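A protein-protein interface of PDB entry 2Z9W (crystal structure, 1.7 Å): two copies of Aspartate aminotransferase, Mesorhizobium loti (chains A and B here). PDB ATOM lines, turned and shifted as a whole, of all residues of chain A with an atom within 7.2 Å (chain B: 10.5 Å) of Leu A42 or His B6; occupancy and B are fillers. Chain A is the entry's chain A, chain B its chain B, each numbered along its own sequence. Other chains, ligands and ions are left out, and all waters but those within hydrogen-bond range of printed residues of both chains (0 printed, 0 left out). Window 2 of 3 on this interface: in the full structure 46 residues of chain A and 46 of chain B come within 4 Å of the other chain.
Leu A42 touches just one residue of chain B: His B6 (3.8 Å).
His B6 touches two residues of chain A.
No residue of chain B comes within 4 Å of Leu A43.
No residue of chain B comes within 4 Å of Glu A45.
No residue of chain B comes within 4 Å of Arg A240.
Of the printed residues of chain A, Arg B324 touches Asp A37, Pro A38 and Ala A39.
Printed residues of chain B within 4 Å of Ala A39: Glu B5 (3.3 Å), His B6 (3.8 Å), Ala B7 (3.8 Å), Asp B8 (3.99 Å) and Arg B324 (3.8 Å).
Of the printed residues of chain A, Pro B9 touches Leu A33 and Asp A37.
The nearest residue of chain B that does not touch Leu A42 is Glu B5 (5.8 Å).
The nearest residue of chain A that does not touch His B6 is Pro A38 (5.3 Å).
The nearest printed residue of chain B that does not touch Pro A38 is His B6 (5.3 Å).
N of Ala A39 lies within hydrogen-bond range of O of Glu B5 (3.3 Å).
The side-chain carboxylate of Asp A37 lies within salt-bridge range of the guanidinium group of Arg B324, at 2.8 Å.
CD1 of Leu A33 touches OD1 of Asp B8, 3.9 Å away.
Pro B9 touches Leu A33.
Pro B9 touches Asp A37.
CG of Pro A38 touches O of Glu B5, at 3.5 Å.
Pro A38 touches Arg B324 (CD to NE, 3.7 Å).
Ala A39 touches His B6 (CB to O, 3.8 Å).
CB of Ala A39 touches O of Ala B7 (3.8 Å).
Asp B8 touches Ala A39.
Arg B324 touches Ala A39 (NH2 to CB, 3.8 Å).
Leu A42 touches His B6 (CD2 to CB, 3.8 Å).
The backbone carbonyl oxygen (O) of Pro B4 is in hydrogen-bond range of the guanidinium group (NH1) of Arg B324, 3.1 Å away.
The guanidinium group of Arg B324 lies within hydrogen-bond range of the backbone carbonyl oxygen of Ala B7, 2.7 Å away.
The backbone NH (N) of Ala A39 is in hydrogen-bond range of the side-chain carboxylate (OD1) of Asp A37.
Printed residues of chain A that touch a printed residue of chain B: Leu A33, Asp A37, Pro A38, Ala A39 and Leu A42.
Hydrophobic or aromatic side chains of chain A within 4 Å of the printed part of chain B: Leu A33, Pro A38, Ala A39 and Leu A42.
Of the 11 printed residues of chain B, 6 touch a printed residue of chain A.
Hydrophobic or aromatic side chains of chain B that line the printed part of chain A: His B6 and Pro B9.
No position is printed for both chains.
Of the 12 pairs that touch across the chains among the printed residues, none has its exchanged pair printed and touching as well.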
ATOM      1  N   LEU A  33       5.166  34.957 -13.056  1.00  0.00           N
ATOM      2  CA  LEU A  33       3.906  34.318 -13.414  1.00  0.00           C
ATOM      3  C   LEU A  33       3.625  33.106 -12.529  1.00  0.00           C
ATOM      4  O   LEU A  33       4.542  32.507 -11.958  1.00  0.00           O
ATOM      5  CB  LEU A  33       3.925  33.887 -14.880  1.00  0.00           C
ATOM      6  CG  LEU A  33       4.065  35.005 -15.930  1.00  0.00           C
ATOM      7  CD1 LEU A  33       4.056  34.399 -17.320  1.00  0.00           C
ATOM      8  CD2 LEU A  33       2.969  36.066 -15.766  1.00  0.00           C
ATOM      9  N   ASP A  35       3.209  29.370 -12.098  1.00  0.00           N
ATOM     10  CA  ASP A  35       3.937  28.335 -12.866  1.00  0.00           C
ATOM     11  C   ASP A  35       3.029  27.543 -13.805  1.00  0.00           C
ATOM     12  O   ASP A  35       3.472  27.025 -14.832  1.00  0.00           O
ATOM     13  CB  ASP A  35       4.802  27.434 -11.962  1.00  0.00           C
ATOM     14  CG  ASP A  35       4.019  26.761 -10.829  1.00  0.00           C
ATOM     15  OD1 ASP A  35       2.842  27.095 -10.577  1.00  0.00           O
ATOM     16  OD2 ASP A  35       4.619  25.881 -10.186  1.00  0.00           O
ATOM     17  N   ASP A  37       0.454  29.059 -15.298  1.00  0.00           N
ATOM     18  CA  ASP A  37       0.010  29.969 -16.352  1.00  0.00           C
ATOM     19  C   ASP A  37       0.548  29.397 -17.677  1.00  0.00           C
ATOM     20  O   ASP A  37       1.712  28.986 -17.736  1.00  0.00           O
ATOM     21  CB  ASP A  37       0.553  31.367 -16.109  1.00  0.00           C
ATOM     22  CG  ASP A  37       0.005  32.378 -17.092  1.00  0.00           C
ATOM     23  OD1 ASP A  37       0.399  32.345 -18.276  1.00  0.00           O
ATOM     24  OD2 ASP A  37      -0.815  33.216 -16.672  1.00  0.00           O
ATOM     25  N   PRO A  38      -0.299  29.327 -18.722  1.00  0.00           N
ATOM     26  CA  PRO A  38       0.189  28.761 -19.987  1.00  0.00           C
ATOM     27  C   PRO A  38       1.413  29.482 -20.570  1.00  0.00           C
ATOM     28  O   PRO A  38       2.214  28.845 -21.260  1.00  0.00           O
ATOM     29  CB  PRO A  38      -1.018  28.881 -20.924  1.00  0.00           C
ATOM     30  CG  PRO A  38      -1.890  29.944 -20.308  1.00  0.00           C
ATOM     31  CD  PRO A  38      -1.714  29.738 -18.824  1.00  0.00           C
ATOM     32  N   ALA A  39       1.565  30.779 -20.285  1.00  0.00           N
ATOM     33  CA  ALA A  39       2.723  31.523 -20.782  1.00  0.00           C
ATOM     34  C   ALA A  39       4.000  31.079 -20.088  1.00  0.00           C
ATOM     35  O   ALA A  39       5.080  31.074 -20.706  1.00  0.00           O
ATOM     36  CB  ALA A  39       2.532  33.031 -20.628  1.00  0.00           C
ATOM     37  N   PHE A  40       3.893  30.717 -18.813  1.00  0.00           N
ATOM     38  CA  PHE A  40       5.066  30.190 -18.120  1.00  0.00           C
ATOM     39  C   PHE A  40       5.380  28.752 -18.536  1.00  0.00           C
ATOM     40  O   PHE A  40       6.550  28.398 -18.729  1.00  0.00           O
ATOM     41  CB  PHE A  40       4.969  30.290 -16.609  1.00  0.00           C
ATOM     42  CG  PHE A  40       6.242  29.875 -15.927  1.00  0.00           C
ATOM     43  CD1 PHE A  40       6.402  28.574 -15.461  1.00  0.00           C
ATOM     44  CD2 PHE A  40       7.318  30.768 -15.839  1.00  0.00           C
ATOM     45  CE1 PHE A  40       7.597  28.177 -14.859  1.00  0.00           C
ATOM     46  CE2 PHE A  40       8.512  30.387 -15.251  1.00  0.00           C
ATOM     47  CZ  PHE A  40       8.657  29.089 -14.757  1.00  0.00           C
ATOM     48  N   GLN A  41       4.340  27.932 -18.693  1.00  0.00           N
ATOM     49  CA  GLN A  41       4.501  26.561 -19.166  1.00  0.00           C
ATOM     50  C   GLN A  41       5.243  26.537 -20.505  1.00  0.00           C
ATOM     51  O   GLN A  41       6.145  25.720 -20.710  1.00  0.00           O
ATOM     52  CB  GLN A  41       3.139  25.879 -19.287  1.00  0.00           C
ATOM     53  CG  GLN A  41       2.525  25.476 -17.934  1.00  0.00           C
ATOM     54  CD  GLN A  41       3.189  24.232 -17.348  1.00  0.00           C
ATOM     55  OE1 GLN A  41       4.416  24.157 -17.235  1.00  0.00           O
ATOM     56  NE2 GLN A  41       2.377  23.251 -16.971  1.00  0.00           N
ATOM     57  N   LEU A  42       4.866  27.445 -21.401  1.00  0.00           N
ATOM     58  CA  LEU A  42       5.549  27.569 -22.691  1.00  0.00           C
ATOM     59  C   LEU A  42       6.992  28.032 -22.515  1.00  0.00           C
ATOM     60  O   LEU A  42       7.915  27.442 -23.110  1.00  0.00           O
ATOM     61  CB  LEU A  42       4.784  28.529 -23.602  1.00  0.00           C
ATOM     62  CG  LEU A  42       5.242  28.677 -25.046  1.00  0.00           C
ATOM     63  CD1 LEU A  42       5.209  27.343 -25.781  1.00  0.00           C
ATOM     64  CD2 LEU A  42       4.363  29.732 -25.720  1.00  0.00           C
ATOM     65  N   LEU A  43       7.181  29.080 -21.703  1.00  0.00           N
ATOM     66  CA  LEU A  43       8.512  29.637 -21.439  1.00  0.00           C
ATOM     67  C   LEU A  43       9.448  28.560 -20.900  1.00  0.00           C
ATOM     68  O   LEU A  43      10.586  28.418 -21.368  1.00  0.00           O
ATOM     69  CB  LEU A  43       8.463  30.811 -20.442  1.00  0.00           C
ATOM     70  CG  LEU A  43       9.858  31.328 -20.028  1.00  0.00           C
ATOM     71  CD1 LEU A  43      10.345  32.354 -21.032  1.00  0.00           C
ATOM     72  CD2 LEU A  43       9.903  31.895 -18.611  1.00  0.00           C
ATOM     73  N   TYR A  44       8.967  27.807 -19.912  1.00  0.00           N
ATOM     74  CA  TYR A  44       9.782  26.763 -19.297  1.00  0.00           C
ATOM     75  C   TYR A  44      10.228  25.730 -20.340  1.00  0.00           C
ATOM     76  O   TYR A  44      11.404  25.336 -20.378  1.00  0.00           O
ATOM     77  CB  TYR A  44       9.022  26.082 -18.154  1.00  0.00           C
ATOM     78  CG  TYR A  44       9.912  25.253 -17.267  1.00  0.00           C
ATOM     79  CD1 TYR A  44      10.213  23.927 -17.591  1.00  0.00           C
ATOM     80  CD2 TYR A  44      10.479  25.810 -16.112  1.00  0.00           C
ATOM     81  CE1 TYR A  44      11.044  23.161 -16.780  1.00  0.00           C
ATOM     82  CE2 TYR A  44      11.314  25.059 -15.290  1.00  0.00           C
ATOM     83  CZ  TYR A  44      11.588  23.729 -15.629  1.00  0.00           C
ATOM     84  OH  TYR A  44      12.401  22.979 -14.816  1.00  0.00           O
ATOM     85  N   GLU A  45       9.294  25.307 -21.188  1.00  0.00           N
ATOM     86  CA  GLU A  45       9.606  24.336 -22.244  1.00  0.00           C
ATOM     87  C   GLU A  45      10.671  24.888 -23.181  1.00  0.00           C
ATOM     88  O   GLU A  45      11.628  24.179 -23.535  1.00  0.00           O
ATOM     89  CB  GLU A  45       8.352  23.981 -23.052  1.00  0.00           C
ATOM     90  CG  GLU A  45       8.583  22.814 -24.017  1.00  0.00           C
ATOM     91  CD  GLU A  45       7.327  22.417 -24.756  1.00  0.00           C
ATOM     92  OE1 GLU A  45       6.276  22.217 -24.107  1.00  0.00           O
ATOM     93  OE2 GLU A  45       7.392  22.307 -26.000  1.00  0.00           O
ATOM     94  N   LYS A  46      10.496  26.152 -23.554  1.00  0.00           N
ATOM     95  CA  LYS A  46      11.435  26.865 -24.432  1.00  0.00           C
ATOM     96  C   LYS A  46      12.818  27.014 -23.801  1.00  0.00           C
ATOM     97  O   LYS A  46      13.837  26.994 -24.496  1.00  0.00           O
ATOM     98  CB  LYS A  46      10.888  28.247 -24.808  1.00  0.00           C
ATOM     99  CG  LYS A  46       9.824  28.229 -25.906  1.00  0.00           C
ATOM    100  CD  LYS A  46       9.249  29.627 -26.161  1.00  0.00           C
ATOM    101  CE  LYS A  46       8.296  30.057 -25.041  1.00  0.00           C
ATOM    102  NZ  LYS A  46       8.039  31.520 -24.874  1.00  0.00           N
ATOM    103  N   VAL A  47      12.857  27.188 -22.480  1.00  0.00           N
ATOM    104  CA  VAL A  47      14.162  27.270 -21.785  1.00  0.00           C
ATOM    105  C   VAL A  47      14.878  25.924 -21.851  1.00  0.00           C
ATOM    106  O   VAL A  47      16.079  25.866 -22.084  1.00  0.00           O
ATOM    107  CB  VAL A  47      14.041  27.747 -20.302  1.00  0.00           C
ATOM    108  CG1 VAL A  47      15.365  27.585 -19.541  1.00  0.00           C
ATOM    109  CG2 VAL A  47      13.627  29.217 -20.253  1.00  0.00           C
ATOM    110  N   VAL A  48      14.146  24.840 -21.644  1.00  0.00           N
ATOM    111  CA  VAL A  48      14.740  23.515 -21.777  1.00  0.00           C
ATOM    112  C   VAL A  48      15.261  23.328 -23.216  1.00  0.00           C
ATOM    113  O   VAL A  48      16.364  22.789 -23.407  1.00  0.00           O
ATOM    114  CB  VAL A  48      13.760  22.385 -21.363  1.00  0.00           C
ATOM    115  CG1 VAL A  48      14.385  21.005 -21.616  1.00  0.00           C
ATOM    116  CG2 VAL A  48      13.368  22.525 -19.848  1.00  0.00           C
ATOM    117  N   ASP A  49      14.491  23.788 -24.207  1.00  0.00           N
ATOM    118  CA  ASP A  49      14.927  23.709 -25.623  1.00  0.00           C
ATOM    119  C   ASP A  49      16.245  24.466 -25.832  1.00  0.00           C
ATOM    120  O   ASP A  49      17.143  23.968 -26.505  1.00  0.00           O
ATOM    121  CB  ASP A  49      13.875  24.296 -26.583  1.00  0.00           C
ATOM    122  CG  ASP A  49      12.643  23.420 -26.743  1.00  0.00           C
ATOM    123  OD1 ASP A  49      12.688  22.215 -26.423  1.00  0.00           O
ATOM    124  OD2 ASP A  49      11.612  23.960 -27.209  1.00  0.00           O
ATOM    125  N   TRP A 238       9.688  19.266 -18.372  1.00  0.00           N
ATOM    126  CA  TRP A 238      10.007  20.183 -19.473  1.00  0.00           C
ATOM    127  C   TRP A 238       8.755  20.548 -20.279  1.00  0.00           C
ATOM    128  O   TRP A 238       8.665  21.646 -20.848  1.00  0.00           O
ATOM    129  CB  TRP A 238      11.075  19.545 -20.397  1.00  0.00           C
ATOM    130  CG  TRP A 238      10.616  18.238 -21.003  1.00  0.00           C
ATOM    131  CD1 TRP A 238      10.868  16.983 -20.530  1.00  0.00           C
ATOM    132  CD2 TRP A 238       9.798  18.077 -22.164  1.00  0.00           C
ATOM    133  NE1 TRP A 238      10.260  16.043 -21.331  1.00  0.00           N
ATOM    134  CE2 TRP A 238       9.598  16.684 -22.345  1.00  0.00           C
ATOM    135  CE3 TRP A 238       9.233  18.970 -23.086  1.00  0.00           C
ATOM    136  CZ2 TRP A 238       8.835  16.159 -23.414  1.00  0.00           C
ATOM    137  CZ3 TRP A 238       8.460  18.446 -24.143  1.00  0.00           C
ATOM    138  CH2 TRP A 238       8.279  17.054 -24.296  1.00  0.00           C
ATOM    139  N   SER A 239       7.781  19.636 -20.305  1.00  0.00           N
ATOM    140  CA  SER A 239       6.618  19.787 -21.186  1.00  0.00           C
ATOM    141  C   SER A 239       5.568  20.762 -20.658  1.00  0.00           C
ATOM    142  O   SER A 239       5.148  20.662 -19.504  1.00  0.00           O
ATOM    143  CB  SER A 239       5.955  18.436 -21.438  1.00  0.00           C
ATOM    144  OG  SER A 239       4.705  18.628 -22.094  1.00  0.00           O
ATOM    145  N   ARG A 240       5.105  21.661 -21.529  1.00  0.00           N
ATOM    146  CA  ARG A 240       4.057  22.643 -21.187  1.00  0.00           C
ATOM    147  C   ARG A 240       2.739  22.011 -20.716  1.00  0.00           C
ATOM    148  O   ARG A 240       1.886  22.696 -20.137  1.00  0.00           O
ATOM    149  CB  ARG A 240       3.765  23.551 -22.388  1.00  0.00           C
ATOM    150  CG  ARG A 240       3.000  22.846 -23.513  1.00  0.00           C
ATOM    151  CD  ARG A 240       2.879  23.695 -24.758  1.00  0.00           C
ATOM    152  NE  ARG A 240       4.084  23.614 -25.580  1.00  0.00           N
ATOM    153  CZ  ARG A 240       4.204  24.151 -26.792  1.00  0.00           C
ATOM    154  NH1 ARG A 240       3.193  24.824 -27.337  1.00  0.00           N
ATOM    155  NH2 ARG A 240       5.343  24.032 -27.455  1.00  0.00           N
ATOM    156  N   ASP A 241       2.567  20.720 -20.988  1.00  0.00           N
ATOM    157  CA  ASP A 241       1.340  20.003 -20.616  1.00  0.00           C
ATOM    158  C   ASP A 241       1.477  19.166 -19.340  1.00  0.00           C
ATOM    159  O   ASP A 241       0.579  18.387 -18.997  1.00  0.00           O
ATOM    160  CB  ASP A 241       0.893  19.108 -21.778  1.00  0.00           C
ATOM    161  CG  ASP A 241       0.397  19.904 -22.970  1.00  0.00           C
ATOM    162  OD1 ASP A 241      -0.314  20.915 -22.767  1.00  0.00           O
ATOM    163  OD2 ASP A 241       0.718  19.512 -24.110  1.00  0.00           O
ATOM    164  N   ARG B   2     -10.055  38.043 -26.936  1.00  0.00           N
ATOM    165  CA  ARG B   2      -9.551  36.878 -26.215  1.00  0.00           C
ATOM    166  C   ARG B   2      -8.063  37.052 -25.937  1.00  0.00           C
ATOM    167  O   ARG B   2      -7.318  37.530 -26.804  1.00  0.00           O
ATOM    168  CB  ARG B   2      -9.798  35.588 -27.015  1.00  0.00           C
ATOM    169  CG  ARG B   2     -11.278  35.230 -27.286  1.00  0.00           C
ATOM    170  CD  ARG B   2     -12.122  35.131 -26.005  1.00  0.00           C
ATOM    171  NE  ARG B   2     -13.419  34.502 -26.249  1.00  0.00           N
ATOM    172  CZ  ARG B   2     -13.777  33.308 -25.785  1.00  0.00           C
ATOM    173  NH1 ARG B   2     -14.980  32.819 -26.071  1.00  0.00           N
ATOM    174  NH2 ARG B   2     -12.942  32.599 -25.032  1.00  0.00           N
ATOM    175  N   TYR B   3      -7.636  36.675 -24.732  1.00  0.00           N
ATOM    176  CA  TYR B   3      -6.226  36.691 -24.371  1.00  0.00           C
ATOM    177  C   TYR B   3      -5.570  35.393 -24.808  1.00  0.00           C
ATOM    178  O   TYR B   3      -5.976  34.315 -24.384  1.00  0.00           O
ATOM    179  CB  TYR B   3      -6.049  36.910 -22.864  1.00  0.00           C
ATOM    180  CG  TYR B   3      -6.471  38.297 -22.453  1.00  0.00           C
ATOM    181  CD1 TYR B   3      -7.783  38.572 -22.081  1.00  0.00           C
ATOM    182  CD2 TYR B   3      -5.562  39.356 -22.498  1.00  0.00           C
ATOM    183  CE1 TYR B   3      -8.180  39.868 -21.747  1.00  0.00           C
ATOM    184  CE2 TYR B   3      -5.940  40.638 -22.164  1.00  0.00           C
ATOM    185  CZ  TYR B   3      -7.248  40.895 -21.774  1.00  0.00           C
ATOM    186  OH  TYR B   3      -7.619  42.180 -21.439  1.00  0.00           O
ATOM    187  N   PRO B   4      -4.559  35.488 -25.688  1.00  0.00           N
ATOM    188  CA  PRO B   4      -3.847  34.289 -26.109  1.00  0.00           C
ATOM    189  C   PRO B   4      -3.108  33.634 -24.942  1.00  0.00           C
ATOM    190  O   PRO B   4      -2.579  34.327 -24.055  1.00  0.00           O
ATOM    191  CB  PRO B   4      -2.830  34.823 -27.123  1.00  0.00           C
ATOM    192  CG  PRO B   4      -3.394  36.123 -27.596  1.00  0.00           C
ATOM    193  CD  PRO B   4      -4.041  36.693 -26.356  1.00  0.00           C
ATOM    194  N   GLU B   5      -3.061  32.307 -24.964  1.00  0.00           N
ATOM    195  CA  GLU B   5      -2.353  31.531 -23.945  1.00  0.00           C
ATOM    196  C   GLU B   5      -0.851  31.817 -23.916  1.00  0.00           C
ATOM    197  O   GLU B   5      -0.225  31.744 -22.854  1.00  0.00           O
ATOM    198  CB  GLU B   5      -2.589  30.034 -24.159  1.00  0.00           C
ATOM    199  CG  GLU B   5      -3.963  29.556 -23.729  1.00  0.00           C
ATOM    200  CD  GLU B   5      -4.141  28.056 -23.902  1.00  0.00           C
ATOM    201  OE1 GLU B   5      -3.134  27.345 -24.142  1.00  0.00           O
ATOM    202  OE2 GLU B   5      -5.295  27.588 -23.801  1.00  0.00           O
ATOM    203  N   HIS B   6      -0.278  32.138 -25.080  1.00  0.00           N
ATOM    204  CA  HIS B   6       1.165  32.395 -25.187  1.00  0.00           C
ATOM    205  C   HIS B   6       1.562  33.776 -24.675  1.00  0.00           C
ATOM    206  O   HIS B   6       2.710  33.989 -24.290  1.00  0.00           O
ATOM    207  CB  HIS B   6       1.659  32.212 -26.630  1.00  0.00           C
ATOM    208  CG  HIS B   6       1.252  33.321 -27.560  1.00  0.00           C
ATOM    209  ND1 HIS B   6       0.191  33.210 -28.433  1.00  0.00           N
ATOM    210  CD2 HIS B   6       1.771  34.560 -27.757  1.00  0.00           C
ATOM    211  CE1 HIS B   6       0.064  34.333 -29.119  1.00  0.00           C
ATOM    212  NE2 HIS B   6       1.006  35.170 -28.722  1.00  0.00           N
ATOM    213  N   ALA B   7       0.610  34.705 -24.666  1.00  0.00           N
ATOM    214  CA  ALA B   7       0.857  36.074 -24.224  1.00  0.00           C
ATOM    215  C   ALA B   7       0.651  36.189 -22.716  1.00  0.00           C
ATOM    216  O   ALA B   7      -0.058  35.380 -22.129  1.00  0.00           O
ATOM    217  CB  ALA B   7      -0.058  37.026 -24.957  1.00  0.00           C
ATOM    218  N   ASP B   8       1.291  37.181 -22.102  1.00  0.00           N
ATOM    219  CA  ASP B   8       1.199  37.395 -20.654  1.00  0.00           C
ATOM    220  C   ASP B   8      -0.220  37.793 -20.229  1.00  0.00           C
ATOM    221  O   ASP B   8      -0.964  38.397 -21.006  1.00  0.00           O
ATOM    222  CB  ASP B   8       2.224  38.446 -20.171  1.00  0.00           C
ATOM    223  CG  ASP B   8       3.604  37.841 -19.866  1.00  0.00           C
ATOM    224  OD1 ASP B   8       3.939  36.762 -20.406  1.00  0.00           O
ATOM    225  OD2 ASP B   8       4.366  38.454 -19.069  1.00  0.00           O
ATOM    226  N   PRO B   9      -0.611  37.440 -18.990  1.00  0.00           N
ATOM    227  CA  PRO B   9      -1.951  37.834 -18.548  1.00  0.00           C
ATOM    228  C   PRO B   9      -1.974  39.275 -18.065  1.00  0.00           C
ATOM    229  O   PRO B   9      -0.929  39.942 -18.054  1.00  0.00           O
ATOM    230  CB  PRO B   9      -2.201  36.890 -17.378  1.00  0.00           C
ATOM    231  CG  PRO B   9      -0.846  36.778 -16.744  1.00  0.00           C
ATOM    232  CD  PRO B   9       0.104  36.687 -17.938  1.00  0.00           C
ATOM    233  N   VAL B  10      -3.138  39.739 -17.612  1.00  0.00           N
ATOM    234  CA  VAL B  10      -3.282  41.112 -17.158  1.00  0.00           C
ATOM    235  C   VAL B  10      -3.099  41.203 -15.646  1.00  0.00           C
ATOM    236  O   VAL B  10      -2.306  42.022 -15.158  1.00  0.00           O
ATOM    237  CB  VAL B  10      -4.630  41.729 -17.602  1.00  0.00           C
ATOM    238  CG1 VAL B  10      -4.751  43.172 -17.112  1.00  0.00           C
ATOM    239  CG2 VAL B  10      -4.754  41.663 -19.118  1.00  0.00           C
ATOM    240  N   ARG B 324      -9.042  33.575 -17.728  1.00  0.00           N
ATOM    241  CA  ARG B 324      -7.831  34.154 -18.323  1.00  0.00           C
ATOM    242  C   ARG B 324      -8.111  34.586 -19.761  1.00  0.00           C
ATOM    243  O   ARG B 324      -7.698  35.668 -20.176  1.00  0.00           O
ATOM    244  CB  ARG B 324      -6.663  33.168 -18.270  1.00  0.00           C
ATOM    245  CG  ARG B 324      -5.301  33.800 -18.563  1.00  0.00           C
ATOM    246  CD  ARG B 324      -4.238  32.707 -18.706  1.00  0.00           C
ATOM    247  NE  ARG B 324      -2.859  33.206 -18.808  1.00  0.00           N
ATOM    248  CZ  ARG B 324      -2.311  33.700 -19.928  1.00  0.00           C
ATOM    249  NH1 ARG B 324      -3.025  33.825 -21.044  1.00  0.00           N
ATOM    250  NH2 ARG B 324      -1.044  34.085 -19.925  1.00  0.00           N
ATOM    251  N   ALA B 325      -8.812  33.743 -20.519  1.00  0.00           N
ATOM    252  CA  ALA B 325      -9.032  34.024 -21.937  1.00  0.00           C
ATOM    253  C   ALA B 325      -9.942  35.228 -22.130  1.00  0.00           C
ATOM    254  O   ALA B 325      -9.734  36.014 -23.049  1.00  0.00           O
ATOM    255  CB  ALA B 325      -9.605  32.799 -22.666  1.00  0.00           C
